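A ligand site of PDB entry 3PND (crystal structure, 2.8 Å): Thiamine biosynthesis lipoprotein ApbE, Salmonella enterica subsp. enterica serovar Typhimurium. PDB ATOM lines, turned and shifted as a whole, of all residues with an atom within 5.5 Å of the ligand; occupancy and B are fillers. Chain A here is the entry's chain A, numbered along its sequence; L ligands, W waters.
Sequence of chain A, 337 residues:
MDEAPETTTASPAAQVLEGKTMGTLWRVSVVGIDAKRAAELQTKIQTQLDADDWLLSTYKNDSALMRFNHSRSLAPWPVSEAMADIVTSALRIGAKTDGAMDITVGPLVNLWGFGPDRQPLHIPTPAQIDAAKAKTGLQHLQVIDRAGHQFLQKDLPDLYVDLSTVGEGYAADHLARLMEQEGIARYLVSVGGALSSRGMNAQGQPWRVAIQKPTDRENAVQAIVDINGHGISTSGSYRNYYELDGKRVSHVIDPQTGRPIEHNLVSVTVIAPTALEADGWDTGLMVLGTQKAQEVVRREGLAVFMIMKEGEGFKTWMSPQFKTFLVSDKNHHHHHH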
ATOM      1  N   THR A  21      23.784  -2.096  26.727  1.00  0.00           N
ATOM      2  CA  THR A  21      22.455  -2.133  27.313  1.00  0.00           C
ATOM      3  C   THR A  21      21.735  -0.832  27.007  1.00  0.00           C
ATOM      4  O   THR A  21      22.369   0.215  26.868  1.00  0.00           O
ATOM      5  CB  THR A  21      22.497  -2.389  28.857  1.00  0.00           C
ATOM      6  OG1 THR A  21      21.158  -2.553  29.352  1.00  0.00           O
ATOM      7  CG2 THR A  21      23.179  -1.231  29.594  1.00  0.00           C
ATOM      8  N   MET A  22      20.414  -0.913  26.862  1.00  0.00           N
ATOM      9  CA  MET A  22      19.559   0.268  26.726  1.00  0.00           C
ATOM     10  C   MET A  22      20.013   1.204  25.601  1.00  0.00           C
ATOM     11  O   MET A  22      19.964   2.421  25.762  1.00  0.00           O
ATOM     12  CB  MET A  22      19.498   1.031  28.055  1.00  0.00           C
ATOM     13  CG  MET A  22      18.988   0.213  29.229  1.00  0.00           C
ATOM     14  SD  MET A  22      19.204   1.069  30.809  1.00  0.00           S
ATOM     15  CE  MET A  22      18.283  -0.002  31.897  1.00  0.00           C
ATOM     16  N   GLY A  23      20.444   0.637  24.482  1.00  0.00           N
ATOM     17  CA  GLY A  23      20.922   1.432  23.339  1.00  0.00           C
ATOM     18  C   GLY A  23      22.141   2.290  23.620  1.00  0.00           C
ATOM     19  O   GLY A  23      22.352   3.306  22.951  1.00  0.00           O
ATOM     20  N   THR A  24      22.927   1.899  24.625  1.00  0.00           N
ATOM     21  CA  THR A  24      24.161   2.600  24.989  1.00  0.00           C
ATOM     22  C   THR A  24      25.174   1.606  25.570  1.00  0.00           C
ATOM     23  O   THR A  24      24.976   0.388  25.472  1.00  0.00           O
ATOM     24  CB  THR A  24      23.888   3.806  25.948  1.00  0.00           C
ATOM     25  OG1 THR A  24      25.094   4.535  26.170  1.00  0.00           O
ATOM     26  CG2 THR A  24      23.298   3.350  27.289  1.00  0.00           C
ATOM     27  N   ASP A  52      16.493  -4.634  33.812  1.00  0.00           N
ATOM     28  CA  ASP A  52      16.271  -3.192  33.976  1.00  0.00           C
ATOM     29  C   ASP A  52      15.760  -2.566  32.675  1.00  0.00           C
ATOM     30  O   ASP A  52      14.905  -1.686  32.696  1.00  0.00           O
ATOM     31  CB  ASP A  52      17.546  -2.493  34.438  1.00  0.00           C
ATOM     32  CG  ASP A  52      17.951  -2.858  35.857  1.00  0.00           C
ATOM     33  OD1 ASP A  52      17.116  -3.430  36.601  1.00  0.00           O
ATOM     34  OD2 ASP A  52      19.109  -2.592  36.237  1.00  0.00           O
ATOM     35  N   ASP A  53      16.321  -3.030  31.552  1.00  0.00           N
ATOM     36  CA  ASP A  53      15.887  -2.632  30.217  1.00  0.00           C
ATOM     37  C   ASP A  53      14.427  -3.061  29.986  1.00  0.00           C
ATOM     38  O   ASP A  53      13.622  -2.294  29.468  1.00  0.00           O
ATOM     39  CB  ASP A  53      16.795  -3.286  29.161  1.00  0.00           C
ATOM     40  CG  ASP A  53      16.742  -2.607  27.802  1.00  0.00           C
ATOM     41  OD1 ASP A  53      15.888  -1.725  27.579  1.00  0.00           O
ATOM     42  OD2 ASP A  53      17.568  -2.963  26.944  1.00  0.00           O
ATOM     43  N   LEU A  56      12.062  -0.629  32.126  1.00  0.00           N
ATOM     44  CA  LEU A  56      12.042   0.827  31.950  1.00  0.00           C
ATOM     45  C   LEU A  56      12.027   1.353  30.517  1.00  0.00           C
ATOM     46  O   LEU A  56      11.793   2.542  30.288  1.00  0.00           O
ATOM     47  CB  LEU A  56      13.230   1.457  32.711  1.00  0.00           C
ATOM     48  CG  LEU A  56      13.417   1.182  34.207  1.00  0.00           C
ATOM     49  CD1 LEU A  56      14.754   1.723  34.671  1.00  0.00           C
ATOM     50  CD2 LEU A  56      12.259   1.759  35.031  1.00  0.00           C
ATOM     51  N   SER A  57      12.267   0.470  29.544  1.00  0.00           N
ATOM     52  CA  SER A  57      12.441   0.896  28.144  1.00  0.00           C
ATOM     53  C   SER A  57      11.177   1.461  27.513  1.00  0.00           C
ATOM     54  O   SER A  57      10.080   0.943  27.719  1.00  0.00           O
ATOM     55  CB  SER A  57      12.965  -0.265  27.298  1.00  0.00           C
ATOM     56  OG  SER A  57      13.262   0.171  25.977  1.00  0.00           O
ATOM     57  N   THR A  58      11.356   2.542  26.748  1.00  0.00           N
ATOM     58  CA  THR A  58      10.293   3.099  25.896  1.00  0.00           C
ATOM     59  C   THR A  58      10.369   2.525  24.487  1.00  0.00           C
ATOM     60  O   THR A  58       9.456   2.709  23.684  1.00  0.00           O
ATOM     61  CB  THR A  58      10.341   4.645  25.833  1.00  0.00           C
ATOM     62  OG1 THR A  58      11.670   5.073  25.518  1.00  0.00           O
ATOM     63  CG2 THR A  58       9.921   5.267  27.155  1.00  0.00           C
ATOM     64  N   TYR A  59      11.468   1.826  24.201  1.00  0.00           N
ATOM     65  CA  TYR A  59      11.726   1.236  22.888  1.00  0.00           C
ATOM     66  C   TYR A  59      11.269  -0.220  22.798  1.00  0.00           C
ATOM     67  O   TYR A  59      11.441  -0.875  21.774  1.00  0.00           O
ATOM     68  CB  TYR A  59      13.231   1.347  22.559  1.00  0.00           C
ATOM     69  CG  TYR A  59      13.728   2.765  22.435  1.00  0.00           C
ATOM     70  CD1 TYR A  59      14.038   3.313  21.188  1.00  0.00           C
ATOM     71  CD2 TYR A  59      13.896   3.568  23.564  1.00  0.00           C
ATOM     72  CE1 TYR A  59      14.495   4.629  21.077  1.00  0.00           C
ATOM     73  CE2 TYR A  59      14.353   4.880  23.463  1.00  0.00           C
ATOM     74  CZ  TYR A  59      14.652   5.397  22.214  1.00  0.00           C
ATOM     75  OH  TYR A  59      15.098   6.696  22.118  1.00  0.00           O
ATOM     76  N   ALA A 100      10.910  21.378  35.328  1.00  0.00           N
ATOM     77  CA  ALA A 100      11.875  21.363  34.222  1.00  0.00           C
ATOM     78  C   ALA A 100      12.113  19.953  33.676  1.00  0.00           C
ATOM     79  O   ALA A 100      11.954  19.727  32.480  1.00  0.00           O
ATOM     80  CB  ALA A 100      13.184  21.990  34.651  1.00  0.00           C
ATOM     81  N   MET A 101      12.475  19.015  34.552  1.00  0.00           N
ATOM     82  CA  MET A 101      12.558  17.622  34.148  1.00  0.00           C
ATOM     83  C   MET A 101      11.238  16.933  34.507  1.00  0.00           C
ATOM     84  O   MET A 101      10.890  16.782  35.682  1.00  0.00           O
ATOM     85  CB  MET A 101      13.821  16.927  34.700  1.00  0.00           C
ATOM     86  CG  MET A 101      13.605  15.853  35.764  1.00  0.00           C
ATOM     87  SD  MET A 101      13.055  14.294  35.062  1.00  0.00           S
ATOM     88  CE  MET A 101      13.073  13.267  36.527  1.00  0.00           C
ATOM     89  N   ASP A 102      10.504  16.541  33.467  1.00  0.00           N
ATOM     90  CA  ASP A 102       9.132  16.092  33.600  1.00  0.00           C
ATOM     91  C   ASP A 102       8.999  14.734  32.923  1.00  0.00           C
ATOM     92  O   ASP A 102       9.092  14.636  31.699  1.00  0.00           O
ATOM     93  CB  ASP A 102       8.209  17.118  32.910  1.00  0.00           C
ATOM     94  CG  ASP A 102       6.740  16.888  33.188  1.00  0.00           C
ATOM     95  OD1 ASP A 102       6.349  15.744  33.539  1.00  0.00           O
ATOM     96  OD2 ASP A 102       5.969  17.855  33.035  1.00  0.00           O
ATOM     97  N   ILE A 103       8.788  13.695  33.712  1.00  0.00           N
ATOM     98  CA  ILE A 103       8.702  12.332  33.175  1.00  0.00           C
ATOM     99  C   ILE A 103       7.399  12.057  32.417  1.00  0.00           C
ATOM    100  O   ILE A 103       7.231  10.971  31.867  1.00  0.00           O
ATOM    101  CB  ILE A 103       8.925  11.257  34.267  1.00  0.00           C
ATOM    102  CG1 ILE A 103       7.878  11.363  35.377  1.00  0.00           C
ATOM    103  CG2 ILE A 103      10.352  11.330  34.803  1.00  0.00           C
ATOM    104  CD1 ILE A 103       7.697  10.094  36.191  1.00  0.00           C
ATOM    105  N   VAL A 105       6.584  14.048  29.888  1.00  0.00           N
ATOM    106  CA  VAL A 105       6.831  14.773  28.646  1.00  0.00           C
ATOM    107  C   VAL A 105       6.756  13.857  27.398  1.00  0.00           C
ATOM    108  O   VAL A 105       6.945  14.315  26.268  1.00  0.00           O
ATOM    109  CB  VAL A 105       8.191  15.552  28.718  1.00  0.00           C
ATOM    110  CG1 VAL A 105       9.373  14.624  28.431  1.00  0.00           C
ATOM    111  CG2 VAL A 105       8.192  16.759  27.791  1.00  0.00           C
ATOM    112  N   VAL A 109       7.769  14.232  23.321  1.00  0.00           N
ATOM    113  CA  VAL A 109       8.893  13.468  22.778  1.00  0.00           C
ATOM    114  C   VAL A 109       8.466  12.725  21.509  1.00  0.00           C
ATOM    115  O   VAL A 109       9.182  12.728  20.495  1.00  0.00           O
ATOM    116  CB  VAL A 109       9.469  12.484  23.837  1.00  0.00           C
ATOM    117  CG1 VAL A 109      10.413  11.466  23.208  1.00  0.00           C
ATOM    118  CG2 VAL A 109      10.182  13.257  24.940  1.00  0.00           C
ATOM    119  N   PHE A 114      11.508  12.033  18.876  1.00  0.00           N
ATOM    120  CA  PHE A 114      12.771  11.833  19.587  1.00  0.00           C
ATOM    121  C   PHE A 114      12.852  10.479  20.286  1.00  0.00           C
ATOM    122  O   PHE A 114      13.917  10.086  20.771  1.00  0.00           O
ATOM    123  CB  PHE A 114      13.016  12.969  20.599  1.00  0.00           C
ATOM    124  CG  PHE A 114      13.238  14.310  19.975  1.00  0.00           C
ATOM    125  CD1 PHE A 114      13.854  14.435  18.729  1.00  0.00           C
ATOM    126  CD2 PHE A 114      12.842  15.468  20.639  1.00  0.00           C
ATOM    127  CE1 PHE A 114      14.063  15.683  18.155  1.00  0.00           C
ATOM    128  CE2 PHE A 114      13.050  16.722  20.078  1.00  0.00           C
ATOM    129  CZ  PHE A 114      13.666  16.838  18.829  1.00  0.00           C
ATOM    130  N   ASP A 162       7.862   8.798  30.416  1.00  0.00           N
ATOM    131  CA  ASP A 162       9.175   8.559  29.825  1.00  0.00           C
ATOM    132  C   ASP A 162      10.250   8.703  30.890  1.00  0.00           C
ATOM    133  O   ASP A 162      10.403   9.756  31.501  1.00  0.00           O
ATOM    134  CB  ASP A 162       9.419   9.556  28.683  1.00  0.00           C
ATOM    135  CG  ASP A 162      10.698   9.274  27.913  1.00  0.00           C
ATOM    136  OD1 ASP A 162      11.068  10.097  27.060  1.00  0.00           O
ATOM    137  OD2 ASP A 162      11.342   8.230  28.144  1.00  0.00           O
ATOM    138  N   LEU A 163      10.985   7.613  31.113  1.00  0.00           N
ATOM    139  CA  LEU A 163      12.014   7.588  32.166  1.00  0.00           C
ATOM    140  C   LEU A 163      13.433   7.518  31.593  1.00  0.00           C
ATOM    141  O   LEU A 163      14.362   7.055  32.253  1.00  0.00           O
ATOM    142  CB  LEU A 163      11.758   6.421  33.129  1.00  0.00           C
ATOM    143  CG  LEU A 163      10.415   6.340  33.867  1.00  0.00           C
ATOM    144  CD1 LEU A 163      10.343   5.068  34.701  1.00  0.00           C
ATOM    145  CD2 LEU A 163      10.170   7.558  34.738  1.00  0.00           C
ATOM    146  N   SER A 164      13.581   8.009  30.364  1.00  0.00           N
ATOM    147  CA  SER A 164      14.871   8.013  29.657  1.00  0.00           C
ATOM    148  C   SER A 164      15.965   8.727  30.440  1.00  0.00           C
ATOM    149  O   SER A 164      17.115   8.274  30.451  1.00  0.00           O
ATOM    150  CB  SER A 164      14.729   8.663  28.279  1.00  0.00           C
ATOM    151  OG  SER A 164      13.808   7.958  27.461  1.00  0.00           O
ATOM    152  N   THR A 165      15.621   9.826  31.098  1.00  0.00           N
ATOM    153  CA  THR A 165      16.591  10.660  31.797  1.00  0.00           C
ATOM    154  C   THR A 165      16.845  10.226  33.241  1.00  0.00           C
ATOM    155  O   THR A 165      17.405  10.973  34.043  1.00  0.00           O
ATOM    156  CB  THR A 165      16.206  12.158  31.753  1.00  0.00           C
ATOM    157  OG1 THR A 165      17.310  12.947  32.212  1.00  0.00           O
ATOM    158  CG2 THR A 165      14.988  12.426  32.630  1.00  0.00           C
ATOM    159  N   GLY A 167      16.736   6.318  33.827  1.00  0.00           N
ATOM    160  CA  GLY A 167      17.017   4.893  33.685  1.00  0.00           C
ATOM    161  C   GLY A 167      18.471   4.497  33.872  1.00  0.00           C
ATOM    162  O   GLY A 167      18.770   3.589  34.657  1.00  0.00           O
ATOM    163  N   GLU A 168      19.372   5.176  33.162  1.00  0.00           N
ATOM    164  CA  GLU A 168      20.812   4.905  33.265  1.00  0.00           C
ATOM    165  C   GLU A 168      21.332   5.168  34.667  1.00  0.00           C
ATOM    166  O   GLU A 168      22.219   4.466  35.161  1.00  0.00           O
ATOM    167  CB  GLU A 168      21.607   5.748  32.264  1.00  0.00           C
ATOM    168  CG  GLU A 168      21.415   5.374  30.798  1.00  0.00           C
ATOM    169  CD  GLU A 168      20.292   6.150  30.127  1.00  0.00           C
ATOM    170  OE1 GLU A 168      20.315   6.258  28.887  1.00  0.00           O
ATOM    171  OE2 GLU A 168      19.398   6.655  30.831  1.00  0.00           O
ATOM    172  N   ARG A 248      23.158  19.744  17.463  1.00  0.00           N
ATOM    173  CA  ARG A 248      21.885  19.372  16.832  1.00  0.00           C
ATOM    174  C   ARG A 248      20.704  19.985  17.581  1.00  0.00           C
ATOM    175  O   ARG A 248      20.855  20.433  18.719  1.00  0.00           O
ATOM    176  CB  ARG A 248      21.726  17.849  16.786  1.00  0.00           C
ATOM    177  CG  ARG A 248      21.647  17.199  18.166  1.00  0.00           C
ATOM    178  CD  ARG A 248      21.095  15.798  18.120  1.00  0.00           C
ATOM    179  NE  ARG A 248      21.100  15.179  19.454  1.00  0.00           N
ATOM    180  CZ  ARG A 248      20.820  13.907  19.703  1.00  0.00           C
ATOM    181  NH1 ARG A 248      20.509  13.067  18.719  1.00  0.00           N
ATOM    182  NH2 ARG A 248      20.861  13.458  20.953  1.00  0.00           N
ATOM    183  N   HIS A 251      17.150  17.069  21.867  1.00  0.00           N
ATOM    184  CA  HIS A 251      16.141  16.049  22.154  1.00  0.00           C
ATOM    185  C   HIS A 251      15.548  16.274  23.551  1.00  0.00           C
ATOM    186  O   HIS A 251      14.586  15.612  23.941  1.00  0.00           O
ATOM    187  CB  HIS A 251      16.760  14.649  22.041  1.00  0.00           C
ATOM    188  CG  HIS A 251      16.886  14.164  20.626  1.00  0.00           C
ATOM    189  ND1 HIS A 251      17.323  14.958  19.598  1.00  0.00           N
ATOM    190  CD2 HIS A 251      16.639  12.944  20.085  1.00  0.00           C
ATOM    191  CE1 HIS A 251      17.334  14.269  18.472  1.00  0.00           C
ATOM    192  NE2 HIS A 251      16.922  13.035  18.745  1.00  0.00           N
ATOM    193  N   VAL A 252      16.132  17.229  24.281  1.00  0.00           N
ATOM    194  CA  VAL A 252      15.626  17.655  25.577  1.00  0.00           C
ATOM    195  C   VAL A 252      14.549  18.727  25.360  1.00  0.00           C
ATOM    196  O   VAL A 252      14.802  19.780  24.773  1.00  0.00           O
ATOM    197  CB  VAL A 252      16.762  18.185  26.489  1.00  0.00           C
ATOM    198  CG1 VAL A 252      16.221  18.599  27.842  1.00  0.00           C
ATOM    199  CG2 VAL A 252      17.853  17.130  26.660  1.00  0.00           C
ATOM    200  N   ILE A 253      13.352  18.451  25.859  1.00  0.00           N
ATOM    201  CA  ILE A 253      12.178  19.292  25.625  1.00  0.00           C
ATOM    202  C   ILE A 253      11.804  20.106  26.860  1.00  0.00           C
ATOM    203  O   ILE A 253      11.759  19.578  27.967  1.00  0.00           O
ATOM    204  CB  ILE A 253      10.969  18.462  25.120  1.00  0.00           C
ATOM    205  CG1 ILE A 253      11.256  17.932  23.703  1.00  0.00           C
ATOM    206  CG2 ILE A 253       9.683  19.282  25.135  1.00  0.00           C
ATOM    207  CD1 ILE A 253      10.279  16.893  23.218  1.00  0.00           C
ATOM    208  N   ASP A 254      11.558  21.396  26.646  1.00  0.00           N
ATOM    209  CA  ASP A 254      11.041  22.290  27.674  1.00  0.00           C
ATOM    210  C   ASP A 254       9.527  22.064  27.789  1.00  0.00           C
ATOM    211  O   ASP A 254       8.785  22.386  26.859  1.00  0.00           O
ATOM    212  CB  ASP A 254      11.349  23.743  27.311  1.00  0.00           C
ATOM    213  CG  ASP A 254      10.937  24.741  28.386  1.00  0.00           C
ATOM    214  OD1 ASP A 254      10.413  24.338  29.442  1.00  0.00           O
ATOM    215  OD2 ASP A 254      11.145  25.949  28.161  1.00  0.00           O
ATOM    216  N   PRO A 255       9.067  21.494  28.930  1.00  0.00           N
ATOM    217  CA  PRO A 255       7.648  21.131  29.111  1.00  0.00           C
ATOM    218  C   PRO A 255       6.717  22.342  29.149  1.00  0.00           C
ATOM    219  O   PRO A 255       5.503  22.198  29.044  1.00  0.00           O
ATOM    220  CB  PRO A 255       7.641  20.436  30.480  1.00  0.00           C
ATOM    221  CG  PRO A 255       9.064  20.106  30.773  1.00  0.00           C
ATOM    222  CD  PRO A 255       9.864  21.184  30.125  1.00  0.00           C
ATOM    223  N   ASP A 279      21.409  11.859  37.248  1.00  0.00           N
ATOM    224  CA  ASP A 279      20.820  11.672  35.922  1.00  0.00           C
ATOM    225  C   ASP A 279      19.583  12.539  35.723  1.00  0.00           C
ATOM    226  O   ASP A 279      19.403  13.139  34.655  1.00  0.00           O
ATOM    227  CB  ASP A 279      20.465  10.189  35.713  1.00  0.00           C
ATOM    228  CG  ASP A 279      20.333   9.806  34.249  1.00  0.00           C
ATOM    229  OD1 ASP A 279      20.836  10.547  33.378  1.00  0.00           O
ATOM    230  OD2 ASP A 279      19.738   8.751  33.973  1.00  0.00           O
ATOM    231  N   THR A 283      19.379  16.997  33.334  1.00  0.00           N
ATOM    232  CA  THR A 283      18.374  17.337  32.323  1.00  0.00           C
ATOM    233  C   THR A 283      17.545  18.542  32.775  1.00  0.00           C
ATOM    234  O   THR A 283      17.353  19.488  32.013  1.00  0.00           O
ATOM    235  CB  THR A 283      17.453  16.137  31.998  1.00  0.00           C
ATOM    236  OG1 THR A 283      18.204  15.143  31.275  1.00  0.00           O
ATOM    237  CG2 THR A 283      16.273  16.557  31.128  1.00  0.00           C
ATOM    238  N   VAL A 287      17.306  22.151  30.875  1.00  0.00           N
ATOM    239  CA  VAL A 287      16.026  22.775  30.520  1.00  0.00           C
ATOM    240  C   VAL A 287      15.938  24.200  31.073  1.00  0.00           C
ATOM    241  O   VAL A 287      15.479  25.109  30.382  1.00  0.00           O
ATOM    242  CB  VAL A 287      14.824  21.933  31.026  1.00  0.00           C
ATOM    243  CG1 VAL A 287      13.509  22.682  30.820  1.00  0.00           C
ATOM    244  CG2 VAL A 287      14.763  20.595  30.331  1.00  0.00           C
HETATM  245  P1  LIG L   1      19.187  11.188  27.316  1.00  0.00           P
HETATM  246  O1  LIG L   1      18.502   9.975  26.728  1.00  0.00           O
HETATM  247  O2  LIG L   1      19.790  10.868  28.662  1.00  0.00           O
HETATM  248  O3  LIG L   1      18.137  12.413  27.445  1.00  0.00           O
HETATM  249  C1  LIG L   1      17.295  12.798  26.390  1.00  0.00           C
HETATM  250  C2  LIG L   1      15.989  12.021  26.494  1.00  0.00           C
HETATM  251  O4  LIG L   1      15.285  12.387  27.666  1.00  0.00           O
HETATM  252  C3  LIG L   1      15.070  12.266  25.318  1.00  0.00           C
HETATM  253  O5  LIG L   1      15.241  11.248  24.353  1.00  0.00           O
HETATM  254  C4  LIG L   1      13.679  12.254  25.917  1.00  0.00           C
HETATM  255  O6  LIG L   1      13.085  10.993  25.769  1.00  0.00           O
HETATM  256  C5  LIG L   1      13.891  12.536  27.405  1.00  0.00           C
HETATM  257  N1  LIG L   1      13.471  13.900  27.758  1.00  0.00           N
HETATM  258  C6  LIG L   1      13.463  15.002  26.942  1.00  0.00           C
HETATM  259  N2  LIG L   1      13.014  16.070  27.643  1.00  0.00           N
HETATM  260  C7  LIG L   1      12.743  15.681  28.898  1.00  0.00           C
HETATM  261  C8  LIG L   1      12.261  16.368  30.003  1.00  0.00           C
HETATM  262  N3  LIG L   1      12.294  17.699  30.031  1.00  0.00           N
HETATM  263  N4  LIG L   1      12.070  15.687  31.190  1.00  0.00           N
HETATM  264  C9  LIG L   1      12.350  14.331  31.266  1.00  0.00           C
HETATM  265  N5  LIG L   1      12.830  13.663  30.168  1.00  0.00           N
HETATM  266  C10 LIG L   1      13.021  14.319  28.992  1.00  0.00           C
HETATM  267  N6  LIG L   1      18.037   4.097  22.700  1.00  0.00           N
HETATM  268  C11 LIG L   1      18.022   3.344  21.538  1.00  0.00           C
HETATM  269  O7  LIG L   1      18.425   3.829  20.480  1.00  0.00           O
HETATM  270  N7  LIG L   1      17.544   2.053  21.550  1.00  0.00           N
HETATM  271  C12 LIG L   1      17.081   1.505  22.719  1.00  0.00           C
HETATM  272  O8  LIG L   1      16.663   0.347  22.720  1.00  0.00           O
HETATM  273  C13 LIG L   1      17.095   2.250  23.899  1.00  0.00           C
HETATM  274  N8  LIG L   1      16.632   1.693  25.065  1.00  0.00           N
HETATM  275  C14 LIG L   1      16.636   2.419  26.238  1.00  0.00           C
HETATM  276  C15 LIG L   1      16.165   1.830  27.402  1.00  0.00           C
HETATM  277  C16 LIG L   1      16.167   2.537  28.599  1.00  0.00           C
HETATM  278  C17 LIG L   1      15.639   1.857  29.832  1.00  0.00           C
HETATM  279  C18 LIG L   1      16.641   3.856  28.630  1.00  0.00           C
HETATM  280  C19 LIG L   1      16.655   4.653  29.904  1.00  0.00           C
HETATM  281  C20 LIG L   1      17.114   4.439  27.453  1.00  0.00           C
HETATM  282  C21 LIG L   1      17.122   3.736  26.247  1.00  0.00           C
HETATM  283  N9  LIG L   1      17.596   4.319  25.070  1.00  0.00           N
HETATM  284  C22 LIG L   1      17.572   3.573  23.889  1.00  0.00           C
HETATM  285  C23 LIG L   1      18.340   5.635  25.113  1.00  0.00           C
HETATM  286  C24 LIG L   1      19.852   5.401  25.182  1.00  0.00           C
HETATM  287  O9  LIG L   1      20.199   4.978  26.489  1.00  0.00           O
HETATM  288  C25 LIG L   1      20.782   6.564  24.758  1.00  0.00           C
HETATM  289  O10 LIG L   1      21.676   6.885  25.807  1.00  0.00           O
HETATM  290  C26 LIG L   1      20.118   7.854  24.283  1.00  0.00           C
HETATM  291  O11 LIG L   1      19.331   7.609  23.153  1.00  0.00           O
HETATM  292  C27 LIG L   1      21.173   8.880  23.927  1.00  0.00           C
HETATM  293  O12 LIG L   1      21.238   9.833  24.952  1.00  0.00           O
HETATM  294  P2  LIG L   1      20.463  11.237  24.797  1.00  0.00           P
HETATM  295  O13 LIG L   1      21.328  12.199  24.006  1.00  0.00           O
HETATM  296  O14 LIG L   1      19.119  11.061  24.145  1.00  0.00           O
HETATM  297  O15 LIG L   1      20.318  11.760  26.310  1.00  0.00           O
HETATM  298  O   HOH W   1      13.722   4.720  27.610  1.00  0.00           O
HETATM  299  O   HOH W   2      12.744  10.948  30.784  1.00  0.00           O
HETATM  300  O   HOH W   3      19.654   9.249  31.221  1.00  0.00           O
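O of Ile 253 is in hydrogen-bond range of N3 of the ligand (2.8 Å). O of Ala 100 sits at hydrogen-bond distance from N3 of the ligand (3.2 Å). N of Asp 102 is in hydrogen-bond range of N4 of the ligand. The guanidinium group (NH2) of Arg 248 lies within salt-bridge range of an oxygen (O13) of the ligand (3.3 Å). OE1 of Glu 168 lies within hydrogen-bond range of O9 of the ligand. The side-chain carboxylate (OD1) of Asp 162 sits at hydrogen-bond distance from an oxygen (O6) of the ligand (2.6 Å). The backbone NH (N) of Ile 253 sits at hydrogen-bond distance from a nitrogen (N2) of the ligand (3.0 Å). An oxygen (O9) of the ligand is in hydrogen-bond range of the backbone carbonyl oxygen (O) of Met 22 (2.7 Å).
OG of Ser 57 is in hydrogen-bond range of N of Tyr 59 (3.0 Å). O of Asp 279 sits at hydrogen-bond distance from OG1 of Thr 165. OG1 of Thr 165 is in hydrogen-bond range of OG1 of Thr 283 (2.5 Å). The backbone NH (N) of Asp 162 lies within hydrogen-bond range of the backbone carbonyl oxygen (O) of Ile 103, 2.7 Å away. The side-chain hydroxyl (OG) of Ser 164 lies within hydrogen-bond range of the side-chain carboxylate (OD2) of Asp 162 (2.6 Å). The backbone carbonyl oxygen of Val 109 is in hydrogen-bond range of the backbone NH of Phe 114, 2.9 Å away.
Residues that only touch the ligand: His 251, Tyr 59, Thr 165, Ser 164, Val 105, Met 101, Asp 53, Thr 24, Ser 57, Val 252, Leu 56, Val 109, Gly 23, Gly 167, Val 287 and Phe 114. Hydrophobic or aromatic side chains within 4 Å of the ligand: Met 22, Leu 56, Tyr 59, Met 101, Val 105, Val 109 and Val 287. The nearest printed residue that does not touch the ligand is Leu 163 (4.1 Å).
Water W2 lies within hydrogen-bond range of O of Asp 162 (2.7 Å), N5 of the ligand (2.8 Å), N of Ser 164 (3.1 Å) and N of Thr 165 (3.1 Å). Water W1 lies within hydrogen-bond range of the side-chain hydroxyl of Thr 58 (3.0 Å) and the side-chain hydroxyl of Ser 164 (3.2 Å).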
